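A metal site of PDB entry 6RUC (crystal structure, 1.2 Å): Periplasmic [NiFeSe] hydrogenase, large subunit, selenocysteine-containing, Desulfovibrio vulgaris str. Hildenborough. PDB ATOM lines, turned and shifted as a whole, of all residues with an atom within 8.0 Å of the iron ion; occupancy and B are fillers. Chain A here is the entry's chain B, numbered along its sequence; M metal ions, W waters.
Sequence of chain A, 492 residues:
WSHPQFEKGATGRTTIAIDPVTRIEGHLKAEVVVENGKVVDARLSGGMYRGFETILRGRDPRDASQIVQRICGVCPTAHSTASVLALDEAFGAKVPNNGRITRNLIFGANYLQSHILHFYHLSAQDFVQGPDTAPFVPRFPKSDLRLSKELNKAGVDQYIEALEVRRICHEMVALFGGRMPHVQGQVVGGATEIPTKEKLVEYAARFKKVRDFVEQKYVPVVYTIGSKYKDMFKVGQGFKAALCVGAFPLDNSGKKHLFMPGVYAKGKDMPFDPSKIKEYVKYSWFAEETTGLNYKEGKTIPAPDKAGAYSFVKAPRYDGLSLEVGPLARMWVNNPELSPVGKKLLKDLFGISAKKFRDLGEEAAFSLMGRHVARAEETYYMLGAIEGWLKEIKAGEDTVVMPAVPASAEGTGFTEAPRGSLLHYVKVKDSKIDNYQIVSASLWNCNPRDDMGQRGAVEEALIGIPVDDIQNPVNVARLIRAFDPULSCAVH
A ring nitrogen (ND1) of His 492 is in hydrogen-bond range of the backbone carbonyl oxygen (O) of Cys 489 (2.8 Å). The side-chain carboxylate (OE1) of Glu 53 lies within hydrogen-bond range of the side-chain hydroxyl (OG1) of Thr 300, 2.7 Å away. A ring nitrogen (ND1) of His 492 lies close to the backbone carbonyl oxygen (O) of Ala 490 (3.5 Å). The side-chain carboxylate of Glu 53 sits close to the side-chain amide oxygen of Gln 437 (3.4 Å).
Within 4 Å of the iron ion: Glu 53, Ile 438 and His 492. The nearest printed residue that does not touch the iron ion is Glu 279 (4.1 Å).
The iron ion is bound by water W3, a ring nitrogen (NE2) of His 492, water W2, the side-chain carboxylate of Glu 53, water W1 and the backbone carbonyl oxygen of Ile 438.
Water W2 lies within hydrogen-bond range of the side-chain carboxylate (OE1) of Glu 279 (2.6 Å), the side-chain amide oxygen (OE1) of Gln 437 (2.7 Å) and the side-chain amino group (NZ) of Lys 314 (3.1 Å). Water W1 lies within hydrogen-bond range of OE1 of Glu 53 and NZ of Lys 314.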
ATOM      1  N   TYR A  49      -0.572  23.668   9.085  1.00  0.00           N
ATOM      2  CA  TYR A  49       0.591  23.423   9.927  1.00  0.00           C
ATOM      3  C   TYR A  49       0.197  22.570  11.119  1.00  0.00           C
ATOM      4  O   TYR A  49      -0.857  22.791  11.734  1.00  0.00           O
ATOM      5  CB  TYR A  49       1.129  24.767  10.429  1.00  0.00           C
ATOM      6  CG  TYR A  49       2.265  24.677  11.440  1.00  0.00           C
ATOM      7  CD1 TYR A  49       3.581  24.485  11.026  1.00  0.00           C
ATOM      8  CD2 TYR A  49       2.023  24.793  12.806  1.00  0.00           C
ATOM      9  CE1 TYR A  49       4.628  24.418  11.944  1.00  0.00           C
ATOM     10  CE2 TYR A  49       3.069  24.725  13.742  1.00  0.00           C
ATOM     11  CZ  TYR A  49       4.362  24.528  13.293  1.00  0.00           C
ATOM     12  OH  TYR A  49       5.427  24.474  14.183  1.00  0.00           O
ATOM     13  N   GLU A  53       8.013  19.036  14.491  1.00  0.00           N
ATOM     14  CA  GLU A  53       9.345  19.285  15.052  1.00  0.00           C
ATOM     15  C   GLU A  53       9.288  19.759  16.495  1.00  0.00           C
ATOM     16  O   GLU A  53      10.299  19.661  17.203  1.00  0.00           O
ATOM     17  CB  GLU A  53      10.100  20.271  14.165  1.00  0.00           C
ATOM     18  CG  GLU A  53      10.402  19.673  12.777  1.00  0.00           C
ATOM     19  CD  GLU A  53      10.557  20.676  11.646  1.00  0.00           C
ATOM     20  OE1 GLU A  53       9.979  21.788  11.754  1.00  0.00           O
ATOM     21  OE2 GLU A  53      11.225  20.342  10.617  1.00  0.00           O
ATOM     22  N   ILE A  71       3.318  12.602   9.456  1.00  0.00           N
ATOM     23  CA  ILE A  71       3.480  13.751   8.587  1.00  0.00           C
ATOM     24  C   ILE A  71       2.649  13.548   7.324  1.00  0.00           C
ATOM     25  O   ILE A  71       2.052  14.497   6.822  1.00  0.00           O
ATOM     26  CB  ILE A  71       4.959  13.998   8.253  1.00  0.00           C
ATOM     27  CG1 ILE A  71       5.670  14.535   9.513  1.00  0.00           C
ATOM     28  CG2 ILE A  71       5.100  14.949   7.056  1.00  0.00           C
ATOM     29  CD1 ILE A  71       7.168  14.602   9.414  1.00  0.00           C
ATOM     30  N   GLU A 279      17.662  26.890   5.692  1.00  0.00           N
ATOM     31  CA  GLU A 279      16.235  27.163   5.553  1.00  0.00           C
ATOM     32  C   GLU A 279      15.940  28.615   5.934  1.00  0.00           C
ATOM     33  O   GLU A 279      16.188  29.049   7.061  1.00  0.00           O
ATOM     34  CB  GLU A 279      15.377  26.201   6.399  1.00  0.00           C
ATOM     35  CG  GLU A 279      15.449  24.764   5.917  1.00  0.00           C
ATOM     36  CD  GLU A 279      14.467  23.861   6.637  1.00  0.00           C
ATOM     37  OE1 GLU A 279      14.773  23.435   7.783  1.00  0.00           O
ATOM     38  OE2 GLU A 279      13.390  23.581   6.072  1.00  0.00           O
ATOM     39  N   PHE A 286       7.088  31.928  10.214  1.00  0.00           N
ATOM     40  CA  PHE A 286       7.964  31.562  11.336  1.00  0.00           C
ATOM     41  C   PHE A 286       8.700  32.793  11.818  1.00  0.00           C
ATOM     42  O   PHE A 286       8.902  33.757  11.074  1.00  0.00           O
ATOM     43  CB  PHE A 286       8.950  30.445  10.933  1.00  0.00           C
ATOM     44  CG  PHE A 286       8.231  29.193  10.519  1.00  0.00           C
ATOM     45  CD1 PHE A 286       7.710  28.329  11.478  1.00  0.00           C
ATOM     46  CD2 PHE A 286       7.969  28.934   9.185  1.00  0.00           C
ATOM     47  CE1 PHE A 286       6.984  27.221  11.111  1.00  0.00           C
ATOM     48  CE2 PHE A 286       7.243  27.825   8.818  1.00  0.00           C
ATOM     49  CZ  PHE A 286       6.754  26.970   9.784  1.00  0.00           C
ATOM     50  N   TYR A 295      19.874  22.583   9.099  1.00  0.00           N
ATOM     51  CA  TYR A 295      18.952  21.717   9.845  1.00  0.00           C
ATOM     52  C   TYR A 295      19.542  21.231  11.177  1.00  0.00           C
ATOM     53  O   TYR A 295      18.787  20.964  12.114  1.00  0.00           O
ATOM     54  CB  TYR A 295      18.490  20.528   8.975  1.00  0.00           C
ATOM     55  CG  TYR A 295      19.660  19.703   8.472  1.00  0.00           C
ATOM     56  CD1 TYR A 295      20.216  18.709   9.260  1.00  0.00           C
ATOM     57  CD2 TYR A 295      20.233  19.969   7.237  1.00  0.00           C
ATOM     58  CE1 TYR A 295      21.319  17.994   8.825  1.00  0.00           C
ATOM     59  CE2 TYR A 295      21.336  19.254   6.803  1.00  0.00           C
ATOM     60  CZ  TYR A 295      21.876  18.284   7.603  1.00  0.00           C
ATOM     61  OH  TYR A 295      22.961  17.587   7.169  1.00  0.00           O
ATOM     62  N   GLY A 298      18.340  23.717  13.409  1.00  0.00           N
ATOM     63  CA  GLY A 298      17.044  24.214  12.993  1.00  0.00           C
ATOM     64  C   GLY A 298      16.135  24.518  14.163  1.00  0.00           C
ATOM     65  O   GLY A 298      16.257  23.940  15.247  1.00  0.00           O
ATOM     66  N   LYS A 299      15.220  25.453  13.946  1.00  0.00           N
ATOM     67  CA  LYS A 299      14.248  25.880  14.924  1.00  0.00           C
ATOM     68  C   LYS A 299      12.915  26.085  14.216  1.00  0.00           C
ATOM     69  O   LYS A 299      12.872  26.541  13.069  1.00  0.00           O
ATOM     70  CB  LYS A 299      14.637  27.212  15.574  1.00  0.00           C
ATOM     71  CG  LYS A 299      15.879  27.137  16.408  1.00  0.00           C
ATOM     72  CD  LYS A 299      16.107  28.465  17.137  1.00  0.00           C
ATOM     73  CE  LYS A 299      16.875  28.281  18.439  1.00  0.00           C
ATOM     74  NZ  LYS A 299      16.842  29.531  19.248  1.00  0.00           N
ATOM     75  N   THR A 300      11.837  25.780  14.934  1.00  0.00           N
ATOM     76  CA  THR A 300      10.487  25.865  14.371  1.00  0.00           C
ATOM     77  C   THR A 300       9.609  26.634  15.349  1.00  0.00           C
ATOM     78  O   THR A 300       9.093  26.072  16.322  1.00  0.00           O
ATOM     79  CB  THR A 300       9.974  24.477  14.034  1.00  0.00           C
ATOM     80  OG1 THR A 300      10.936  23.865  13.180  1.00  0.00           O
ATOM     81  CG2 THR A 300       8.608  24.524  13.371  1.00  0.00           C
ATOM     82  N   PHE A 312       3.358  28.280   5.193  1.00  0.00           N
ATOM     83  CA  PHE A 312       3.944  27.524   6.299  1.00  0.00           C
ATOM     84  C   PHE A 312       5.117  26.653   5.858  1.00  0.00           C
ATOM     85  O   PHE A 312       5.704  25.952   6.694  1.00  0.00           O
ATOM     86  CB  PHE A 312       2.870  26.662   6.991  1.00  0.00           C
ATOM     87  CG  PHE A 312       1.894  27.445   7.858  1.00  0.00           C
ATOM     88  CD1 PHE A 312       2.313  28.095   9.009  1.00  0.00           C
ATOM     89  CD2 PHE A 312       0.549  27.491   7.536  1.00  0.00           C
ATOM     90  CE1 PHE A 312       1.419  28.802   9.810  1.00  0.00           C
ATOM     91  CE2 PHE A 312      -0.341  28.185   8.320  1.00  0.00           C
ATOM     92  CZ  PHE A 312       0.102  28.842   9.471  1.00  0.00           C
ATOM     93  N   VAL A 313       5.481  26.670   4.574  1.00  0.00           N
ATOM     94  CA  VAL A 313       6.663  25.981   4.078  1.00  0.00           C
ATOM     95  C   VAL A 313       7.857  26.920   4.276  1.00  0.00           C
ATOM     96  O   VAL A 313       7.792  28.066   3.854  1.00  0.00           O
ATOM     97  CB  VAL A 313       6.491  25.613   2.596  1.00  0.00           C
ATOM     98  CG1 VAL A 313       7.615  24.751   2.132  1.00  0.00           C
ATOM     99  CG2 VAL A 313       5.169  24.891   2.326  1.00  0.00           C
ATOM    100  N   LYS A 314       8.927  26.423   4.903  1.00  0.00           N
ATOM    101  CA  LYS A 314      10.191  27.175   4.937  1.00  0.00           C
ATOM    102  C   LYS A 314      10.807  27.181   3.529  1.00  0.00           C
ATOM    103  O   LYS A 314      10.345  26.478   2.635  1.00  0.00           O
ATOM    104  CB  LYS A 314      11.174  26.542   5.937  1.00  0.00           C
ATOM    105  CG  LYS A 314      10.741  26.571   7.413  1.00  0.00           C
ATOM    106  CD  LYS A 314      11.765  25.894   8.326  1.00  0.00           C
ATOM    107  CE  LYS A 314      11.369  25.896   9.794  1.00  0.00           C
ATOM    108  NZ  LYS A 314      12.233  24.966  10.595  1.00  0.00           N
ATOM    109  N   LEU A 423      15.458  14.379   4.460  1.00  0.00           N
ATOM    110  CA  LEU A 423      16.362  14.124   5.558  1.00  0.00           C
ATOM    111  C   LEU A 423      15.657  14.399   6.874  1.00  0.00           C
ATOM    112  O   LEU A 423      14.797  15.292   6.967  1.00  0.00           O
ATOM    113  CB  LEU A 423      17.671  14.910   5.456  1.00  0.00           C
ATOM    114  CG  LEU A 423      17.592  16.407   5.691  1.00  0.00           C
ATOM    115  CD1 LEU A 423      17.801  16.778   7.174  1.00  0.00           C
ATOM    116  CD2 LEU A 423      18.593  17.153   4.814  1.00  0.00           C
ATOM    117  N   TYR A 436      14.398  17.790  16.638  1.00  0.00           N
ATOM    118  CA  TYR A 436      14.142  16.921  15.496  1.00  0.00           C
ATOM    119  C   TYR A 436      13.773  17.843  14.355  1.00  0.00           C
ATOM    120  O   TYR A 436      12.855  18.652  14.485  1.00  0.00           O
ATOM    121  CB  TYR A 436      13.009  15.941  15.818  1.00  0.00           C
ATOM    122  CG  TYR A 436      13.000  14.696  14.945  1.00  0.00           C
ATOM    123  CD1 TYR A 436      12.629  14.750  13.619  1.00  0.00           C
ATOM    124  CD2 TYR A 436      13.371  13.462  15.465  1.00  0.00           C
ATOM    125  CE1 TYR A 436      12.602  13.607  12.838  1.00  0.00           C
ATOM    126  CE2 TYR A 436      13.358  12.315  14.684  1.00  0.00           C
ATOM    127  CZ  TYR A 436      12.969  12.387  13.358  1.00  0.00           C
ATOM    128  OH  TYR A 436      12.934  11.240  12.588  1.00  0.00           O
ATOM    129  N   GLN A 437      14.514  17.769  13.246  1.00  0.00           N
ATOM    130  CA  GLN A 437      14.279  18.648  12.110  1.00  0.00           C
ATOM    131  C   GLN A 437      14.088  17.831  10.850  1.00  0.00           C
ATOM    132  O   GLN A 437      14.840  16.886  10.579  1.00  0.00           O
ATOM    133  CB  GLN A 437      15.424  19.647  11.951  1.00  0.00           C
ATOM    134  CG  GLN A 437      15.404  20.720  13.035  1.00  0.00           C
ATOM    135  CD  GLN A 437      14.219  21.685  12.909  1.00  0.00           C
ATOM    136  OE1 GLN A 437      13.846  22.104  11.819  1.00  0.00           O
ATOM    137  NE2 GLN A 437      13.649  22.057  14.034  1.00  0.00           N
ATOM    138  N   ILE A 438      13.074  18.203  10.074  1.00  0.00           N
ATOM    139  CA  ILE A 438      12.709  17.506   8.834  1.00  0.00           C
ATOM    140  C   ILE A 438      12.870  18.476   7.673  1.00  0.00           C
ATOM    141  O   ILE A 438      12.353  19.600   7.713  1.00  0.00           O
ATOM    142  CB  ILE A 438      11.280  16.966   8.930  1.00  0.00           C
ATOM    143  CG1 ILE A 438      11.214  15.880  10.006  1.00  0.00           C
ATOM    144  CG2 ILE A 438      10.811  16.436   7.569  1.00  0.00           C
ATOM    145  CD1 ILE A 438      10.120  16.089  10.978  1.00  0.00           C
ATOM    146  N   VAL A 439      13.553  18.029   6.627  1.00  0.00           N
ATOM    147  CA  VAL A 439      13.721  18.769   5.380  1.00  0.00           C
ATOM    148  C   VAL A 439      13.253  17.786   4.300  1.00  0.00           C
ATOM    149  O   VAL A 439      13.962  16.816   3.992  1.00  0.00           O
ATOM    150  CB  VAL A 439      15.172  19.225   5.166  1.00  0.00           C
ATOM    151  CG1 VAL A 439      15.333  19.995   3.868  1.00  0.00           C
ATOM    152  CG2 VAL A 439      15.636  20.077   6.344  1.00  0.00           C
ATOM    153  N   SER A 440      12.043  17.990   3.767  1.00  0.00           N
ATOM    154  CA  SER A 440      11.325  16.997   2.966  1.00  0.00           C
ATOM    155  C   SER A 440      11.264  17.382   1.481  1.00  0.00           C
ATOM    156  O   SER A 440      11.679  18.465   1.056  1.00  0.00           O
ATOM    157  CB  SER A 440       9.913  16.870   3.509  1.00  0.00           C
ATOM    158  OG  SER A 440       9.275  18.121   3.414  1.00  0.00           O
ATOM    159  N   LEU A 443       8.971  20.266   0.416  1.00  0.00           N
ATOM    160  CA  LEU A 443       9.632  21.461   0.908  1.00  0.00           C
ATOM    161  C   LEU A 443      10.571  22.050  -0.156  1.00  0.00           C
ATOM    162  O   LEU A 443      10.513  23.252  -0.437  1.00  0.00           O
ATOM    163  CB  LEU A 443      10.367  21.142   2.198  1.00  0.00           C
ATOM    164  CG  LEU A 443      11.384  22.159   2.668  1.00  0.00           C
ATOM    165  CD1 LEU A 443      10.759  23.407   3.244  1.00  0.00           C
ATOM    166  CD2 LEU A 443      12.302  21.501   3.661  1.00  0.00           C
ATOM    167  N   CYS A 489       3.727  16.908   3.771  1.00  0.00           N
ATOM    168  CA  CYS A 489       5.182  16.718   3.879  1.00  0.00           C
ATOM    169  C   CYS A 489       5.918  18.034   3.932  1.00  0.00           C
ATOM    170  O   CYS A 489       6.890  18.188   4.692  1.00  0.00           O
ATOM    171  CB  CYS A 489       5.722  15.936   2.677  1.00  0.00           C
ATOM    172  SG  CYS A 489       5.621  14.165   2.848  1.00  0.00           S
ATOM    173  N   ALA A 490       5.537  19.000   3.076  1.00  0.00           N
ATOM    174  CA  ALA A 490       6.305  20.236   2.947  1.00  0.00           C
ATOM    175  C   ALA A 490       6.291  21.023   4.249  1.00  0.00           C
ATOM    176  O   ALA A 490       7.307  21.632   4.620  1.00  0.00           O
ATOM    177  CB  ALA A 490       5.742  21.089   1.811  1.00  0.00           C
ATOM    178  N   VAL A 491       5.163  21.035   4.945  1.00  0.00           N
ATOM    179  CA  VAL A 491       5.004  21.850   6.160  1.00  0.00           C
ATOM    180  C   VAL A 491       5.314  21.067   7.434  1.00  0.00           C
ATOM    181  O   VAL A 491       5.949  21.590   8.345  1.00  0.00           O
ATOM    182  CB  VAL A 491       3.571  22.444   6.227  1.00  0.00           C
ATOM    183  CG1 VAL A 491       3.415  23.241   7.527  1.00  0.00           C
ATOM    184  CG2 VAL A 491       3.275  23.309   5.009  1.00  0.00           C
ATOM    185  N   HIS A 492       4.790  19.841   7.544  1.00  0.00           N
ATOM    186  CA  HIS A 492       4.928  19.042   8.763  1.00  0.00           C
ATOM    187  C   HIS A 492       4.601  19.829  10.038  1.00  0.00           C
ATOM    188  O   HIS A 492       3.554  20.533  10.069  1.00  0.00           O
ATOM    189  CB  HIS A 492       6.281  18.252   8.814  1.00  0.00           C
ATOM    190  CG  HIS A 492       7.502  19.033   8.409  1.00  0.00           C
ATOM    191  ND1 HIS A 492       7.859  19.227   7.093  1.00  0.00           N
ATOM    192  CD2 HIS A 492       8.485  19.632   9.143  1.00  0.00           C
ATOM    193  CE1 HIS A 492       8.985  19.922   7.025  1.00  0.00           C
ATOM    194  NE2 HIS A 492       9.384  20.181   8.262  1.00  0.00           N
ATOM    195  OXT HIS A 492       5.345  19.717  11.031  1.00  0.00           O
HETATM  196 FE    FE M   1      11.175  21.257   8.676  1.00  0.00          FE
HETATM  197  O   HOH W   1      10.023  23.010   9.424  1.00  0.00           O
HETATM  198  O   HOH W   2      12.951  22.276   9.295  1.00  0.00           O
HETATM  199  O   HOH W   3      11.255  22.248   6.827  1.00  0.00           O
